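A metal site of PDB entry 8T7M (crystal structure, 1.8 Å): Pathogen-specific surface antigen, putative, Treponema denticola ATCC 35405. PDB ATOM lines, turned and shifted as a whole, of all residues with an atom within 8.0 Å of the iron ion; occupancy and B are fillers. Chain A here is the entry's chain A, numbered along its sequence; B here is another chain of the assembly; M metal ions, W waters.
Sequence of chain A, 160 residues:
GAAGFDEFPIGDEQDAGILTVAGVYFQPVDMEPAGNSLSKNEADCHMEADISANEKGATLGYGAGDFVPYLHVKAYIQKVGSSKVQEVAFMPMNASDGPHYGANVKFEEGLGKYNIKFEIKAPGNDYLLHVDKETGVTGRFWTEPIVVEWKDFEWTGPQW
Merely in contact with the iron ion: Asp 50 (3.96 Å). Within 4 Å of the iron ion: Glu 7, Glu 48, Asp 50 and Asp 97. The nearest printed residue that does not touch the iron ion is Phe 5 (4.4 Å).
The iron ion is bound by the side-chain carboxylate (OE2) of Glu 7, 2.1 Å away. The iron ion is bound by OE2 of Glu 48 (2.1 Å). The iron ion is bound by water W1, at 2.1 Å. The iron ion is bound by OD2 of Asp 97 (2.2 Å). Water W2 binds the iron ion (2.3 Å). Water W3 binds the iron ion (2.4 Å).
Water W2 lies within hydrogen-bond range of OD2 of Asp 50 (2.8 Å) and OE1 of Glu 7 (3.1 Å). Water W1 bridges the side-chain carboxylate of Glu 48 and the side-chain carboxylate of Asp 97.
A ring nitrogen (ND1) of His 100 lies close to the side-chain carboxylate (OE1) of Glu 48 (3.5 Å). The backbone NH (N) of Glu 48 lies within hydrogen-bond range of the backbone carbonyl oxygen (O) of Val 24, 3.0 Å away.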
ATOM      1  N   PHE A   5     -22.457  12.888  -5.619  1.00  0.00           N
ATOM      2  CA  PHE A   5     -23.417  12.916  -6.722  1.00  0.00           C
ATOM      3  C   PHE A   5     -22.816  13.693  -7.888  1.00  0.00           C
ATOM      4  O   PHE A   5     -21.782  14.360  -7.763  1.00  0.00           O
ATOM      5  CB  PHE A   5     -24.754  13.541  -6.298  1.00  0.00           C
ATOM      6  CG  PHE A   5     -24.629  14.904  -5.699  1.00  0.00           C
ATOM      7  CD1 PHE A   5     -24.931  16.028  -6.444  1.00  0.00           C
ATOM      8  CD2 PHE A   5     -24.284  15.059  -4.363  1.00  0.00           C
ATOM      9  CE1 PHE A   5     -24.831  17.294  -5.893  1.00  0.00           C
ATOM     10  CE2 PHE A   5     -24.194  16.318  -3.793  1.00  0.00           C
ATOM     11  CZ  PHE A   5     -24.467  17.438  -4.563  1.00  0.00           C
ATOM     12  N   GLU A   7     -22.559  16.511 -10.661  1.00  0.00           N
ATOM     13  CA  GLU A   7     -22.903  17.905 -10.887  1.00  0.00           C
ATOM     14  C   GLU A   7     -22.484  18.323 -12.283  1.00  0.00           C
ATOM     15  O   GLU A   7     -21.407  17.949 -12.756  1.00  0.00           O
ATOM     16  CB  GLU A   7     -22.222  18.818  -9.871  1.00  0.00           C
ATOM     17  CG  GLU A   7     -22.987  18.927  -8.582  1.00  0.00           C
ATOM     18  CD  GLU A   7     -22.184  19.629  -7.516  1.00  0.00           C
ATOM     19  OE1 GLU A   7     -20.946  19.512  -7.539  1.00  0.00           O
ATOM     20  OE2 GLU A   7     -22.810  20.274  -6.657  1.00  0.00           O
ATOM     21  N   VAL A  24     -23.890  25.431 -11.212  1.00  0.00           N
ATOM     22  CA  VAL A  24     -24.040  24.044 -11.625  1.00  0.00           C
ATOM     23  C   VAL A  24     -25.509  23.645 -11.525  1.00  0.00           C
ATOM     24  O   VAL A  24     -26.325  24.320 -10.892  1.00  0.00           O
ATOM     25  CB  VAL A  24     -23.170  23.064 -10.798  1.00  0.00           C
ATOM     26  CG1 VAL A  24     -21.703  23.462 -10.812  1.00  0.00           C
ATOM     27  CG2 VAL A  24     -23.685  22.947  -9.386  1.00  0.00           C
ATOM     28  N   TYR A  25     -25.832  22.534 -12.165  1.00  0.00           N
ATOM     29  CA  TYR A  25     -27.166  21.969 -12.051  1.00  0.00           C
ATOM     30  C   TYR A  25     -27.073  20.462 -11.996  1.00  0.00           C
ATOM     31  O   TYR A  25     -26.051  19.869 -12.359  1.00  0.00           O
ATOM     32  CB  TYR A  25     -28.087  22.400 -13.201  1.00  0.00           C
ATOM     33  CG  TYR A  25     -27.722  21.820 -14.548  1.00  0.00           C
ATOM     34  CD1 TYR A  25     -26.559  22.210 -15.207  1.00  0.00           C
ATOM     35  CD2 TYR A  25     -28.539  20.874 -15.150  1.00  0.00           C
ATOM     36  CE1 TYR A  25     -26.230  21.671 -16.450  1.00  0.00           C
ATOM     37  CE2 TYR A  25     -28.218  20.346 -16.389  1.00  0.00           C
ATOM     38  CZ  TYR A  25     -27.064  20.739 -17.025  1.00  0.00           C
ATOM     39  OH  TYR A  25     -26.744  20.194 -18.248  1.00  0.00           O
ATOM     40  N   PHE A  26     -28.144  19.853 -11.505  1.00  0.00           N
ATOM     41  CA  PHE A  26     -28.272  18.400 -11.396  1.00  0.00           C
ATOM     42  C   PHE A  26     -29.742  18.101 -11.105  1.00  0.00           C
ATOM     43  O   PHE A  26     -30.592  18.991 -11.183  1.00  0.00           O
ATOM     44  CB  PHE A  26     -27.304  17.838 -10.344  1.00  0.00           C
ATOM     45  CG  PHE A  26     -27.291  18.580  -9.027  1.00  0.00           C
ATOM     46  CD1 PHE A  26     -28.183  18.232  -8.021  1.00  0.00           C
ATOM     47  CD2 PHE A  26     -26.379  19.603  -8.797  1.00  0.00           C
ATOM     48  CE1 PHE A  26     -28.157  18.900  -6.798  1.00  0.00           C
ATOM     49  CE2 PHE A  26     -26.362  20.272  -7.574  1.00  0.00           C
ATOM     50  CZ  PHE A  26     -27.246  19.914  -6.572  1.00  0.00           C
ATOM     51  N   HIS A  46     -32.215  20.929 -10.072  1.00  0.00           N
ATOM     52  CA  HIS A  46     -31.766  21.778  -8.972  1.00  0.00           C
ATOM     53  C   HIS A  46     -30.673  22.670  -9.558  1.00  0.00           C
ATOM     54  O   HIS A  46     -29.807  22.183 -10.301  1.00  0.00           O
ATOM     55  CB  HIS A  46     -31.229  20.964  -7.804  1.00  0.00           C
ATOM     56  CG  HIS A  46     -31.045  21.763  -6.560  1.00  0.00           C
ATOM     57  ND1 HIS A  46     -32.102  22.289  -5.845  1.00  0.00           N
ATOM     58  CD2 HIS A  46     -29.918  22.184  -5.922  1.00  0.00           C
ATOM     59  CE1 HIS A  46     -31.647  22.965  -4.803  1.00  0.00           C
ATOM     60  NE2 HIS A  46     -30.320  22.924  -4.833  1.00  0.00           N
ATOM     61  N   GLU A  48     -27.730  25.711  -8.653  1.00  0.00           N
ATOM     62  CA  GLU A  48     -27.025  26.260  -7.491  1.00  0.00           C
ATOM     63  C   GLU A  48     -25.937  27.240  -7.912  1.00  0.00           C
ATOM     64  O   GLU A  48     -25.344  27.132  -8.998  1.00  0.00           O
ATOM     65  CB  GLU A  48     -26.471  25.118  -6.626  1.00  0.00           C
ATOM     66  CG  GLU A  48     -25.015  24.800  -6.773  1.00  0.00           C
ATOM     67  CD  GLU A  48     -24.645  23.536  -6.001  1.00  0.00           C
ATOM     68  OE1 GLU A  48     -25.510  22.966  -5.300  1.00  0.00           O
ATOM     69  OE2 GLU A  48     -23.477  23.121  -6.097  1.00  0.00           O
ATOM     70  N   ALA A  49     -25.746  28.258  -7.066  1.00  0.00           N
ATOM     71  CA  ALA A  49     -24.611  29.160  -7.111  1.00  0.00           C
ATOM     72  C   ALA A  49     -23.641  28.762  -6.005  1.00  0.00           C
ATOM     73  O   ALA A  49     -23.983  28.862  -4.827  1.00  0.00           O
ATOM     74  CB  ALA A  49     -25.062  30.605  -6.924  1.00  0.00           C
ATOM     75  N   ASP A  50     -22.457  28.269  -6.379  1.00  0.00           N
ATOM     76  CA  ASP A  50     -21.354  28.108  -5.433  1.00  0.00           C
ATOM     77  C   ASP A  50     -20.598  29.421  -5.361  1.00  0.00           C
ATOM     78  O   ASP A  50     -19.918  29.813  -6.317  1.00  0.00           O
ATOM     79  CB  ASP A  50     -20.415  26.969  -5.836  1.00  0.00           C
ATOM     80  CG  ASP A  50     -21.092  25.628  -5.892  1.00  0.00           C
ATOM     81  OD1 ASP A  50     -22.000  25.382  -5.060  1.00  0.00           O
ATOM     82  OD2 ASP A  50     -20.698  24.798  -6.747  1.00  0.00           O
ATOM     83  N   ALA A  95     -26.215  20.727   1.053  1.00  0.00           N
ATOM     84  CA  ALA A  95     -26.293  19.386   0.493  1.00  0.00           C
ATOM     85  C   ALA A  95     -25.163  18.559   1.109  1.00  0.00           C
ATOM     86  O   ALA A  95     -24.431  19.046   1.976  1.00  0.00           O
ATOM     87  CB  ALA A  95     -26.212  19.418  -1.038  1.00  0.00           C
ATOM     88  N   SER A  96     -24.999  17.320   0.641  1.00  0.00           N
ATOM     89  CA  SER A  96     -23.938  16.476   1.189  1.00  0.00           C
ATOM     90  C   SER A  96     -22.556  17.023   0.851  1.00  0.00           C
ATOM     91  O   SER A  96     -21.574  16.653   1.515  1.00  0.00           O
ATOM     92  CB  SER A  96     -24.061  15.041   0.691  1.00  0.00           C
ATOM     93  OG  SER A  96     -24.268  14.998  -0.705  1.00  0.00           O
ATOM     94  N   ASP A  97     -22.455  17.884  -0.148  1.00  0.00           N
ATOM     95  CA  ASP A  97     -21.199  18.476  -0.581  1.00  0.00           C
ATOM     96  C   ASP A  97     -20.982  19.880  -0.014  1.00  0.00           C
ATOM     97  O   ASP A  97     -20.027  20.559  -0.418  1.00  0.00           O
ATOM     98  CB  ASP A  97     -21.145  18.530  -2.103  1.00  0.00           C
ATOM     99  CG  ASP A  97     -22.054  19.591  -2.680  1.00  0.00           C
ATOM    100  OD1 ASP A  97     -23.191  19.757  -2.179  1.00  0.00           O
ATOM    101  OD2 ASP A  97     -21.650  20.248  -3.657  1.00  0.00           O
ATOM    102  N   GLY A  98     -21.859  20.353   0.854  1.00  0.00           N
ATOM    103  CA  GLY A  98     -21.626  21.593   1.560  1.00  0.00           C
ATOM    104  C   GLY A  98     -22.604  22.709   1.256  1.00  0.00           C
ATOM    105  O   GLY A  98     -23.619  22.512   0.584  1.00  0.00           O
ATOM    106  N   PRO A  99     -22.315  23.898   1.767  1.00  0.00           N
ATOM    107  CA  PRO A  99     -23.238  25.027   1.605  1.00  0.00           C
ATOM    108  C   PRO A  99     -23.186  25.607   0.206  1.00  0.00           C
ATOM    109  O   PRO A  99     -22.165  25.552  -0.482  1.00  0.00           O
ATOM    110  CB  PRO A  99     -22.747  26.037   2.637  1.00  0.00           C
ATOM    111  CG  PRO A  99     -21.284  25.755   2.730  1.00  0.00           C
ATOM    112  CD  PRO A  99     -21.156  24.255   2.613  1.00  0.00           C
ATOM    113  N   HIS A 100     -24.315  26.173  -0.212  1.00  0.00           N
ATOM    114  CA  HIS A 100     -24.470  26.810  -1.513  1.00  0.00           C
ATOM    115  C   HIS A 100     -25.773  27.599  -1.467  1.00  0.00           C
ATOM    116  O   HIS A 100     -26.543  27.488  -0.502  1.00  0.00           O
ATOM    117  CB  HIS A 100     -24.477  25.778  -2.643  1.00  0.00           C
ATOM    118  CG  HIS A 100     -25.598  24.783  -2.560  1.00  0.00           C
ATOM    119  ND1 HIS A 100     -25.490  23.601  -1.872  1.00  0.00           N
ATOM    120  CD2 HIS A 100     -26.832  24.787  -3.110  1.00  0.00           C
ATOM    121  CE1 HIS A 100     -26.624  22.928  -1.973  1.00  0.00           C
ATOM    122  NE2 HIS A 100     -27.450  23.619  -2.744  1.00  0.00           N
ATOM    123  N   TYR A 101     -26.029  28.376  -2.503  1.00  0.00           N
ATOM    124  CA  TYR A 101     -27.338  28.974  -2.715  1.00  0.00           C
ATOM    125  C   TYR A 101     -28.004  28.199  -3.840  1.00  0.00           C
ATOM    126  O   TYR A 101     -27.363  27.916  -4.857  1.00  0.00           O
ATOM    127  CB  TYR A 101     -27.241  30.459  -3.090  1.00  0.00           C
ATOM    128  CG  TYR A 101     -26.583  31.319  -2.039  1.00  0.00           C
ATOM    129  CD1 TYR A 101     -25.201  31.423  -1.961  1.00  0.00           C
ATOM    130  CD2 TYR A 101     -27.349  32.025  -1.117  1.00  0.00           C
ATOM    131  CE1 TYR A 101     -24.585  32.226  -0.974  1.00  0.00           C
ATOM    132  CE2 TYR A 101     -26.754  32.822  -0.131  1.00  0.00           C
ATOM    133  CZ  TYR A 101     -25.364  32.922  -0.076  1.00  0.00           C
ATOM    134  OH  TYR A 101     -24.781  33.711   0.906  1.00  0.00           O
ATOM    135  N   HIS B 130     -30.797  19.596   2.089  1.00  0.00           N
ATOM    136  CA  HIS B 130     -31.232  18.549   1.157  1.00  0.00           C
ATOM    137  C   HIS B 130     -31.473  17.288   1.984  1.00  0.00           C
ATOM    138  O   HIS B 130     -30.606  16.881   2.758  1.00  0.00           O
ATOM    139  CB  HIS B 130     -30.187  18.237   0.065  1.00  0.00           C
ATOM    140  CG  HIS B 130     -29.972  19.325  -0.947  1.00  0.00           C
ATOM    141  ND1 HIS B 130     -29.322  19.101  -2.146  1.00  0.00           N
ATOM    142  CD2 HIS B 130     -30.239  20.654  -0.923  1.00  0.00           C
ATOM    143  CE1 HIS B 130     -29.244  20.224  -2.836  1.00  0.00           C
ATOM    144  NE2 HIS B 130     -29.797  21.192  -2.111  1.00  0.00           N
HETATM  145 FE    FE M   1     -22.763  21.500  -5.010  1.00  0.00          FE
HETATM  146 CU    CU M   2     -29.528  23.140  -2.903  1.00  0.00          CU
HETATM  147  O   HOH W   1     -24.644  20.912  -4.242  1.00  0.00           O
HETATM  148  O   HOH W   2     -20.759  22.101  -5.886  1.00  0.00           O
HETATM  149  O   HOH W   3     -22.287  23.078  -3.288  1.00  0.00           O
